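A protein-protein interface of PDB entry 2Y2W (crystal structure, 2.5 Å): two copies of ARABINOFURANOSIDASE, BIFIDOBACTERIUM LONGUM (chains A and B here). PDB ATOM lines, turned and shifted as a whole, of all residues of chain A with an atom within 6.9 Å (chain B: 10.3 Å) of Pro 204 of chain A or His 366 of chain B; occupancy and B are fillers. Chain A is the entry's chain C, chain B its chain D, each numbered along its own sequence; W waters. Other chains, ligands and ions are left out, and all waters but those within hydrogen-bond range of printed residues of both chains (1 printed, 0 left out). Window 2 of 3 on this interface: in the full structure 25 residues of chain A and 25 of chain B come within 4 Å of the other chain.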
ATOM      1  N   TYR A 153     -17.901  17.267   6.993  1.00  0.00           N
ATOM      2  CA  TYR A 153     -18.407  18.637   7.082  1.00  0.00           C
ATOM      3  C   TYR A 153     -18.095  19.230   8.457  1.00  0.00           C
ATOM      4  O   TYR A 153     -17.629  20.367   8.552  1.00  0.00           O
ATOM      5  CB  TYR A 153     -19.913  18.713   6.791  1.00  0.00           C
ATOM      6  CG  TYR A 153     -20.517  20.069   7.104  1.00  0.00           C
ATOM      7  CD1 TYR A 153     -20.324  21.153   6.250  1.00  0.00           C
ATOM      8  CD2 TYR A 153     -21.269  20.271   8.261  1.00  0.00           C
ATOM      9  CE1 TYR A 153     -20.866  22.403   6.537  1.00  0.00           C
ATOM     10  CE2 TYR A 153     -21.814  21.518   8.559  1.00  0.00           C
ATOM     11  CZ  TYR A 153     -21.611  22.576   7.691  1.00  0.00           C
ATOM     12  OH  TYR A 153     -22.148  23.811   7.977  1.00  0.00           O
ATOM     13  N   TYR A 183     -29.372  16.495  -0.499  1.00  0.00           N
ATOM     14  CA  TYR A 183     -29.129  16.222   0.915  1.00  0.00           C
ATOM     15  C   TYR A 183     -28.156  17.231   1.507  1.00  0.00           C
ATOM     16  O   TYR A 183     -28.375  17.756   2.597  1.00  0.00           O
ATOM     17  CB  TYR A 183     -28.588  14.798   1.090  1.00  0.00           C
ATOM     18  CG  TYR A 183     -28.061  14.475   2.476  1.00  0.00           C
ATOM     19  CD1 TYR A 183     -28.929  14.111   3.507  1.00  0.00           C
ATOM     20  CD2 TYR A 183     -26.692  14.520   2.752  1.00  0.00           C
ATOM     21  CE1 TYR A 183     -28.451  13.806   4.779  1.00  0.00           C
ATOM     22  CE2 TYR A 183     -26.201  14.220   4.025  1.00  0.00           C
ATOM     23  CZ  TYR A 183     -27.086  13.864   5.032  1.00  0.00           C
ATOM     24  OH  TYR A 183     -26.609  13.562   6.290  1.00  0.00           O
ATOM     25  N   VAL A 184     -27.090  17.494   0.759  1.00  0.00           N
ATOM     26  CA  VAL A 184     -25.984  18.336   1.187  1.00  0.00           C
ATOM     27  C   VAL A 184     -26.340  19.827   1.202  1.00  0.00           C
ATOM     28  O   VAL A 184     -26.040  20.536   2.170  1.00  0.00           O
ATOM     29  CB  VAL A 184     -24.731  18.035   0.308  1.00  0.00           C
ATOM     30  CG1 VAL A 184     -23.947  19.277  -0.024  1.00  0.00           C
ATOM     31  CG2 VAL A 184     -23.848  16.994   0.980  1.00  0.00           C
ATOM     32  N   ASN A 185     -27.001  20.294   0.146  1.00  0.00           N
ATOM     33  CA  ASN A 185     -27.241  21.723  -0.029  1.00  0.00           C
ATOM     34  C   ASN A 185     -28.698  22.185   0.134  1.00  0.00           C
ATOM     35  O   ASN A 185     -28.964  23.385   0.195  1.00  0.00           O
ATOM     36  CB  ASN A 185     -26.690  22.180  -1.382  1.00  0.00           C
ATOM     37  CG  ASN A 185     -25.174  22.287  -1.394  1.00  0.00           C
ATOM     38  OD1 ASN A 185     -24.528  22.323  -0.346  1.00  0.00           O
ATOM     39  ND2 ASN A 185     -24.599  22.348  -2.588  1.00  0.00           N
ATOM     40  N   GLY A 186     -29.623  21.231   0.220  1.00  0.00           N
ATOM     41  CA  GLY A 186     -31.056  21.522   0.176  1.00  0.00           C
ATOM     42  C   GLY A 186     -31.660  22.241   1.365  1.00  0.00           C
ATOM     43  O   GLY A 186     -31.307  21.984   2.514  1.00  0.00           O
ATOM     44  N   ALA A 187     -32.588  23.147   1.079  1.00  0.00           N
ATOM     45  CA  ALA A 187     -33.338  23.835   2.124  1.00  0.00           C
ATOM     46  C   ALA A 187     -34.261  22.845   2.832  1.00  0.00           C
ATOM     47  O   ALA A 187     -34.822  21.960   2.184  1.00  0.00           O
ATOM     48  CB  ALA A 187     -34.146  24.989   1.528  1.00  0.00           C
ATOM     49  N   PRO A 188     -34.419  22.985   4.164  1.00  0.00           N
ATOM     50  CA  PRO A 188     -35.360  22.130   4.888  1.00  0.00           C
ATOM     51  C   PRO A 188     -36.751  22.160   4.255  1.00  0.00           C
ATOM     52  O   PRO A 188     -37.232  23.224   3.854  1.00  0.00           O
ATOM     53  CB  PRO A 188     -35.393  22.760   6.285  1.00  0.00           C
ATOM     54  CG  PRO A 188     -34.060  23.395   6.430  1.00  0.00           C
ATOM     55  CD  PRO A 188     -33.737  23.931   5.068  1.00  0.00           C
ATOM     56  N   ARG A 196     -30.770  15.428   6.676  1.00  0.00           N
ATOM     57  CA  ARG A 196     -29.593  16.158   7.150  1.00  0.00           C
ATOM     58  C   ARG A 196     -29.868  16.883   8.466  1.00  0.00           C
ATOM     59  O   ARG A 196     -29.064  16.808   9.400  1.00  0.00           O
ATOM     60  CB  ARG A 196     -29.109  17.159   6.100  1.00  0.00           C
ATOM     61  CG  ARG A 196     -27.711  17.693   6.369  1.00  0.00           C
ATOM     62  CD  ARG A 196     -27.598  19.180   6.080  1.00  0.00           C
ATOM     63  NE  ARG A 196     -28.036  19.517   4.731  1.00  0.00           N
ATOM     64  CZ  ARG A 196     -29.040  20.339   4.439  1.00  0.00           C
ATOM     65  NH1 ARG A 196     -29.727  20.943   5.400  1.00  0.00           N
ATOM     66  NH2 ARG A 196     -29.348  20.560   3.170  1.00  0.00           N
ATOM     67  N   ILE A 201     -27.273  18.423  11.352  1.00  0.00           N
ATOM     68  CA  ILE A 201     -26.811  19.574  10.575  1.00  0.00           C
ATOM     69  C   ILE A 201     -28.005  20.277   9.928  1.00  0.00           C
ATOM     70  O   ILE A 201     -28.564  19.795   8.938  1.00  0.00           O
ATOM     71  CB  ILE A 201     -25.772  19.154   9.503  1.00  0.00           C
ATOM     72  CG1 ILE A 201     -24.615  18.383  10.153  1.00  0.00           C
ATOM     73  CG2 ILE A 201     -25.247  20.376   8.747  1.00  0.00           C
ATOM     74  CD1 ILE A 201     -23.826  17.516   9.197  1.00  0.00           C
ATOM     75  N   GLU A 202     -28.396  21.411  10.503  1.00  0.00           N
ATOM     76  CA  GLU A 202     -29.585  22.137  10.055  1.00  0.00           C
ATOM     77  C   GLU A 202     -29.314  22.945   8.788  1.00  0.00           C
ATOM     78  O   GLU A 202     -30.070  22.865   7.815  1.00  0.00           O
ATOM     79  CB  GLU A 202     -30.100  23.052  11.170  1.00  0.00           C
ATOM     80  N   GLU A 203     -28.231  23.717   8.820  1.00  0.00           N
ATOM     81  CA  GLU A 203     -27.832  24.590   7.720  1.00  0.00           C
ATOM     82  C   GLU A 203     -27.314  23.789   6.525  1.00  0.00           C
ATOM     83  O   GLU A 203     -26.754  22.705   6.707  1.00  0.00           O
ATOM     84  CB  GLU A 203     -26.765  25.590   8.201  1.00  0.00           C
ATOM     85  CG  GLU A 203     -25.360  25.001   8.450  1.00  0.00           C
ATOM     86  CD  GLU A 203     -25.191  24.336   9.815  1.00  0.00           C
ATOM     87  OE1 GLU A 203     -26.080  23.569  10.246  1.00  0.00           O
ATOM     88  OE2 GLU A 203     -24.144  24.569  10.456  1.00  0.00           O
ATOM     89  N   PRO A 204     -27.509  24.314   5.297  1.00  0.00           N
ATOM     90  CA  PRO A 204     -26.893  23.698   4.120  1.00  0.00           C
ATOM     91  C   PRO A 204     -25.381  23.634   4.275  1.00  0.00           C
ATOM     92  O   PRO A 204     -24.793  24.480   4.952  1.00  0.00           O
ATOM     93  CB  PRO A 204     -27.254  24.663   2.988  1.00  0.00           C
ATOM     94  CG  PRO A 204     -28.494  25.331   3.442  1.00  0.00           C
ATOM     95  CD  PRO A 204     -28.369  25.456   4.931  1.00  0.00           C
ATOM     96  N   MET A 205     -24.761  22.636   3.661  1.00  0.00           N
ATOM     97  CA  MET A 205     -23.314  22.462   3.750  1.00  0.00           C
ATOM     98  C   MET A 205     -22.561  23.458   2.871  1.00  0.00           C
ATOM     99  O   MET A 205     -21.368  23.685   3.066  1.00  0.00           O
ATOM    100  CB  MET A 205     -22.919  21.020   3.407  1.00  0.00           C
ATOM    101  CG  MET A 205     -23.423  19.992   4.411  1.00  0.00           C
ATOM    102  SD  MET A 205     -22.676  18.368   4.198  1.00  0.00           S
ATOM    103  CE  MET A 205     -23.540  17.424   5.444  1.00  0.00           C
ATOM    104  N   ASP A 206     -23.274  24.055   1.915  1.00  0.00           N
ATOM    105  CA  ASP A 206     -22.710  25.025   0.970  1.00  0.00           C
ATOM    106  C   ASP A 206     -21.533  24.469   0.164  1.00  0.00           C
ATOM    107  O   ASP A 206     -20.524  25.153  -0.050  1.00  0.00           O
ATOM    108  CB  ASP A 206     -22.339  26.345   1.667  1.00  0.00           C
ATOM    109  CG  ASP A 206     -23.555  27.206   1.976  1.00  0.00           C
ATOM    110  OD1 ASP A 206     -24.605  27.021   1.316  1.00  0.00           O
ATOM    111  OD2 ASP A 206     -23.462  28.069   2.879  1.00  0.00           O
ATOM    112  N   ILE A 207     -21.677  23.223  -0.277  1.00  0.00           N
ATOM    113  CA  ILE A 207     -20.702  22.606  -1.161  1.00  0.00           C
ATOM    114  C   ILE A 207     -20.944  23.111  -2.585  1.00  0.00           C
ATOM    115  O   ILE A 207     -21.962  22.809  -3.216  1.00  0.00           O
ATOM    116  CB  ILE A 207     -20.723  21.065  -1.061  1.00  0.00           C
ATOM    117  CG1 ILE A 207     -20.444  20.641   0.388  1.00  0.00           C
ATOM    118  CG2 ILE A 207     -19.702  20.451  -2.018  1.00  0.00           C
ATOM    119  CD1 ILE A 207     -20.545  19.161   0.661  1.00  0.00           C
ATOM    120  N   GLU A 245     -28.840  23.776  -9.492  1.00  0.00           N
ATOM    121  CA  GLU A 245     -28.085  24.844  -8.850  1.00  0.00           C
ATOM    122  C   GLU A 245     -27.059  25.422  -9.819  1.00  0.00           C
ATOM    123  O   GLU A 245     -26.023  24.807 -10.084  1.00  0.00           O
ATOM    124  CB  GLU A 245     -27.400  24.329  -7.574  1.00  0.00           C
ATOM    125  CG  GLU A 245     -26.536  25.361  -6.855  1.00  0.00           C
ATOM    126  CD  GLU A 245     -27.346  26.486  -6.242  1.00  0.00           C
ATOM    127  OE1 GLU A 245     -27.973  26.255  -5.186  1.00  0.00           O
ATOM    128  OE2 GLU A 245     -27.343  27.604  -6.808  1.00  0.00           O
ATOM    129  N   ARG B 135     -37.758  17.155  -5.029  1.00  0.00           N
ATOM    130  CA  ARG B 135     -37.392  18.215  -5.955  1.00  0.00           C
ATOM    131  C   ARG B 135     -37.785  17.823  -7.368  1.00  0.00           C
ATOM    132  O   ARG B 135     -37.701  16.650  -7.739  1.00  0.00           O
ATOM    133  CB  ARG B 135     -35.877  18.419  -5.949  1.00  0.00           C
ATOM    134  CG  ARG B 135     -35.323  19.292  -4.855  1.00  0.00           C
ATOM    135  CD  ARG B 135     -33.816  19.403  -5.023  1.00  0.00           C
ATOM    136  NE  ARG B 135     -33.257  20.545  -4.308  1.00  0.00           N
ATOM    137  CZ  ARG B 135     -31.979  20.906  -4.345  1.00  0.00           C
ATOM    138  NH1 ARG B 135     -31.099  20.213  -5.066  1.00  0.00           N
ATOM    139  NH2 ARG B 135     -31.576  21.967  -3.657  1.00  0.00           N
ATOM    140  N   HIS B 140     -37.926  23.531 -11.482  1.00  0.00           N
ATOM    141  CA  HIS B 140     -37.378  24.107 -10.253  1.00  0.00           C
ATOM    142  C   HIS B 140     -38.450  24.277  -9.178  1.00  0.00           C
ATOM    143  O   HIS B 140     -38.646  25.363  -8.640  1.00  0.00           O
ATOM    144  CB  HIS B 140     -36.655  25.431 -10.544  1.00  0.00           C
ATOM    145  CG  HIS B 140     -35.582  25.764  -9.556  1.00  0.00           C
ATOM    146  ND1 HIS B 140     -34.382  25.086  -9.505  1.00  0.00           N
ATOM    147  CD2 HIS B 140     -35.521  26.706  -8.586  1.00  0.00           C
ATOM    148  CE1 HIS B 140     -33.632  25.594  -8.545  1.00  0.00           C
ATOM    149  NE2 HIS B 140     -34.299  26.580  -7.973  1.00  0.00           N
ATOM    150  N   TRP B 356     -31.578  32.761 -14.843  1.00  0.00           N
ATOM    151  CA  TRP B 356     -31.161  31.711 -13.915  1.00  0.00           C
ATOM    152  C   TRP B 356     -29.704  31.313 -14.161  1.00  0.00           C
ATOM    153  O   TRP B 356     -28.965  31.030 -13.219  1.00  0.00           O
ATOM    154  CB  TRP B 356     -32.095  30.499 -14.048  1.00  0.00           C
ATOM    155  CG  TRP B 356     -31.580  29.217 -13.452  1.00  0.00           C
ATOM    156  CD1 TRP B 356     -31.089  28.138 -14.131  1.00  0.00           C
ATOM    157  CD2 TRP B 356     -31.513  28.880 -12.060  1.00  0.00           C
ATOM    158  NE1 TRP B 356     -30.717  27.151 -13.251  1.00  0.00           N
ATOM    159  CE2 TRP B 356     -30.965  27.579 -11.972  1.00  0.00           C
ATOM    160  CE3 TRP B 356     -31.858  29.549 -10.879  1.00  0.00           C
ATOM    161  CZ2 TRP B 356     -30.756  26.934 -10.749  1.00  0.00           C
ATOM    162  CZ3 TRP B 356     -31.650  28.907  -9.662  1.00  0.00           C
ATOM    163  CH2 TRP B 356     -31.102  27.614  -9.608  1.00  0.00           C
ATOM    164  N   GLU B 359     -27.366  34.053 -13.005  1.00  0.00           N
ATOM    165  CA  GLU B 359     -27.404  34.180 -11.548  1.00  0.00           C
ATOM    166  C   GLU B 359     -26.299  33.331 -10.897  1.00  0.00           C
ATOM    167  O   GLU B 359     -26.200  33.248  -9.669  1.00  0.00           O
ATOM    168  CB  GLU B 359     -28.792  33.780 -11.026  1.00  0.00           C
ATOM    169  CG  GLU B 359     -29.126  34.249  -9.606  1.00  0.00           C
ATOM    170  CD  GLU B 359     -29.320  35.751  -9.498  1.00  0.00           C
ATOM    171  OE1 GLU B 359     -30.171  36.304 -10.231  1.00  0.00           O
ATOM    172  OE2 GLU B 359     -28.628  36.379  -8.666  1.00  0.00           O
ATOM    173  N   GLN B 362     -23.699  35.123  -8.394  1.00  0.00           N
ATOM    174  CA  GLN B 362     -24.142  35.529  -7.057  1.00  0.00           C
ATOM    175  C   GLN B 362     -23.852  34.468  -5.990  1.00  0.00           C
ATOM    176  O   GLN B 362     -23.695  34.797  -4.811  1.00  0.00           O
ATOM    177  CB  GLN B 362     -25.632  35.901  -7.069  1.00  0.00           C
ATOM    178  CG  GLN B 362     -26.089  36.785  -5.898  1.00  0.00           C
ATOM    179  CD  GLN B 362     -25.723  38.261  -6.067  1.00  0.00           C
ATOM    180  OE1 GLN B 362     -26.594  39.105  -6.296  1.00  0.00           O
ATOM    181  NE2 GLN B 362     -24.434  38.575  -5.948  1.00  0.00           N
ATOM    182  N   GLY B 363     -23.777  33.206  -6.408  1.00  0.00           N
ATOM    183  CA  GLY B 363     -23.458  32.104  -5.498  1.00  0.00           C
ATOM    184  C   GLY B 363     -24.518  31.019  -5.468  1.00  0.00           C
ATOM    185  O   GLY B 363     -25.243  30.820  -6.445  1.00  0.00           O
ATOM    186  N   LEU B 364     -24.604  30.316  -4.342  1.00  0.00           N
ATOM    187  CA  LEU B 364     -25.585  29.246  -4.167  1.00  0.00           C
ATOM    188  C   LEU B 364     -26.914  29.794  -3.653  1.00  0.00           C
ATOM    189  O   LEU B 364     -26.955  30.859  -3.027  1.00  0.00           O
ATOM    190  CB  LEU B 364     -25.057  28.173  -3.209  1.00  0.00           C
ATOM    191  CG  LEU B 364     -23.707  27.501  -3.483  1.00  0.00           C
ATOM    192  CD1 LEU B 364     -23.324  26.630  -2.302  1.00  0.00           C
ATOM    193  CD2 LEU B 364     -23.722  26.684  -4.768  1.00  0.00           C
ATOM    194  N   HIS B 365     -27.994  29.059  -3.917  1.00  0.00           N
ATOM    195  CA  HIS B 365     -29.336  29.464  -3.504  1.00  0.00           C
ATOM    196  C   HIS B 365     -29.829  28.626  -2.326  1.00  0.00           C
ATOM    197  O   HIS B 365     -29.863  27.397  -2.398  1.00  0.00           O
ATOM    198  CB  HIS B 365     -30.316  29.372  -4.678  1.00  0.00           C
ATOM    199  CG  HIS B 365     -29.871  30.124  -5.894  1.00  0.00           C
ATOM    200  ND1 HIS B 365     -29.332  29.501  -6.999  1.00  0.00           N
ATOM    201  CD2 HIS B 365     -29.868  31.450  -6.172  1.00  0.00           C
ATOM    202  CE1 HIS B 365     -29.023  30.409  -7.907  1.00  0.00           C
ATOM    203  NE2 HIS B 365     -29.339  31.599  -7.431  1.00  0.00           N
ATOM    204  N   HIS B 366     -30.204  29.305  -1.246  1.00  0.00           N
ATOM    205  CA  HIS B 366     -30.658  28.646  -0.021  1.00  0.00           C
ATOM    206  C   HIS B 366     -32.177  28.516   0.024  1.00  0.00           C
ATOM    207  O   HIS B 366     -32.705  27.660   0.731  1.00  0.00           O
ATOM    208  CB  HIS B 366     -30.186  29.426   1.211  1.00  0.00           C
ATOM    209  CG  HIS B 366     -28.706  29.381   1.440  1.00  0.00           C
ATOM    210  ND1 HIS B 366     -28.155  29.207   2.693  1.00  0.00           N
ATOM    211  CD2 HIS B 366     -27.661  29.496   0.585  1.00  0.00           C
ATOM    212  CE1 HIS B 366     -26.837  29.216   2.599  1.00  0.00           C
ATOM    213  NE2 HIS B 366     -26.512  29.387   1.329  1.00  0.00           N
ATOM    214  N   GLU B 367     -32.869  29.372  -0.721  1.00  0.00           N
ATOM    215  CA  GLU B 367     -34.329  29.438  -0.692  1.00  0.00           C
ATOM    216  C   GLU B 367     -34.975  28.131  -1.152  1.00  0.00           C
ATOM    217  O   GLU B 367     -34.509  27.518  -2.117  1.00  0.00           O
ATOM    218  CB  GLU B 367     -34.832  30.608  -1.547  1.00  0.00           C
ATOM    219  N   PRO B 368     -36.041  27.692  -0.452  1.00  0.00           N
ATOM    220  CA  PRO B 368     -36.780  26.502  -0.870  1.00  0.00           C
ATOM    221  C   PRO B 368     -37.467  26.713  -2.216  1.00  0.00           C
ATOM    222  O   PRO B 368     -37.956  27.810  -2.499  1.00  0.00           O
ATOM    223  CB  PRO B 368     -37.819  26.318   0.242  1.00  0.00           C
ATOM    224  CG  PRO B 368     -37.935  27.650   0.888  1.00  0.00           C
ATOM    225  CD  PRO B 368     -36.574  28.251   0.804  1.00  0.00           C
ATOM    226  N   TRP B 369     -37.483  25.668  -3.035  1.00  0.00           N
ATOM    227  CA  TRP B 369     -38.085  25.726  -4.360  1.00  0.00           C
ATOM    228  C   TRP B 369     -39.603  25.901  -4.220  1.00  0.00           C
ATOM    229  O   TRP B 369     -40.204  25.341  -3.303  1.00  0.00           O
ATOM    230  CB  TRP B 369     -37.727  24.463  -5.154  1.00  0.00           C
ATOM    231  CG  TRP B 369     -36.229  24.250  -5.366  1.00  0.00           C
ATOM    232  CD1 TRP B 369     -35.200  24.874  -4.707  1.00  0.00           C
ATOM    233  CD2 TRP B 369     -35.611  23.324  -6.272  1.00  0.00           C
ATOM    234  NE1 TRP B 369     -33.990  24.407  -5.160  1.00  0.00           N
ATOM    235  CE2 TRP B 369     -34.212  23.455  -6.120  1.00  0.00           C
ATOM    236  CE3 TRP B 369     -36.104  22.404  -7.207  1.00  0.00           C
ATOM    237  CZ2 TRP B 369     -33.300  22.703  -6.868  1.00  0.00           C
ATOM    238  CZ3 TRP B 369     -35.194  21.652  -7.950  1.00  0.00           C
ATOM    239  CH2 TRP B 369     -33.810  21.809  -7.774  1.00  0.00           C
ATOM    240  N   PRO B 370     -40.222  26.710  -5.100  1.00  0.00           N
ATOM    241  CA  PRO B 370     -41.653  27.016  -4.987  1.00  0.00           C
ATOM    242  C   PRO B 370     -42.585  25.821  -5.228  1.00  0.00           C
ATOM    243  O   PRO B 370     -42.289  24.958  -6.053  1.00  0.00           O
ATOM    244  CB  PRO B 370     -41.869  28.084  -6.065  1.00  0.00           C
ATOM    245  CG  PRO B 370     -40.730  27.932  -7.004  1.00  0.00           C
ATOM    246  CD  PRO B 370     -39.577  27.496  -6.167  1.00  0.00           C
HETATM  247  O   HOH W   1     -32.969  23.732  -1.548  1.00  0.00           O
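The side-chain carboxylate of Asp 206 of chain A sits at hydrogen-bond distance from a ring nitrogen (NE2) of His 366 of chain B (3.0 Å).
The side-chain carboxylate of Glu 245 of chain A lies within hydrogen-bond range of a ring nitrogen (ND1) of His 365 of chain B (2.8 Å).
OD1 of Asn 185 of chain A is in hydrogen-bond range of N of Asp 206 of chain A (3.1 Å).
The guanidinium group of Arg 196 of chain A lies within hydrogen-bond range of the backbone carbonyl oxygen of Gly 186 of chain A (2.5 Å).
Among the printed residues, merely in contact across the chains: Gly 186 of chain A with Arg 135 of chain B, Ala 187 of chain A with His 366 of chain B, Ala 187 of chain A with Pro 368 of chain B, Pro 204 of chain A with His 366 of chain B, Asp 206 of chain A with Leu 364 of chain B, Glu 245 of chain A with Trp 356 of chain B, Glu 245 of chain A with Gly 363 of chain B and Glu 245 of chain A with Leu 364 of chain B.
Pro 204 of chain A touches just one residue of chain B: His 366 (3.96 Å).
His 366 of chain B touches three residues of chain A.
Of chain B, only Arg 135 comes within 4 Å of Gly 186 of chain A.
Glu 203 of chain A touches none of the printed residues of chain B.
Printed residues of chain A within 4 Å of Trp 356 of chain B: Glu 245.
Of the printed residues of chain A, Arg 135 of chain B touches Gly 186 (3.9 Å).
Trp 369 of chain B touches none of the printed residues of chain A.
The nearest residue of chain B that does not touch Pro 204 of chain A is His 365 of chain B (6.3 Å).
The nearest residue of chain A that does not touch His 366 of chain B is Glu 245 of chain A (5.5 Å).
Printed residues of chain B that touch a printed residue of chain A: Arg 135, Trp 356, Gly 363, Leu 364, His 365, His 366 and Pro 368.
Hydrophobic or aromatic side chains of chain B within 4 Å of the printed part of chain A: Trp 356, Leu 364, His 365 and His 366.
Printed residues of chain A that touch a printed residue of chain B: Gly 186, Ala 187, Pro 204, Asp 206 and Glu 245.
Hydrophobic or aromatic side chains of chain A within 4 Å of the printed part of chain B: Ala 187 and Pro 204.
No position is printed for both chains.
Of the 10 pairs that touch across the chains among the printed residues, none has its exchanged pair printed and touching as well.
Water W1 bridges N of Ala 187 of chain A (2.7 Å) and NH2 of Arg 135 of chain B (3.1 Å).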
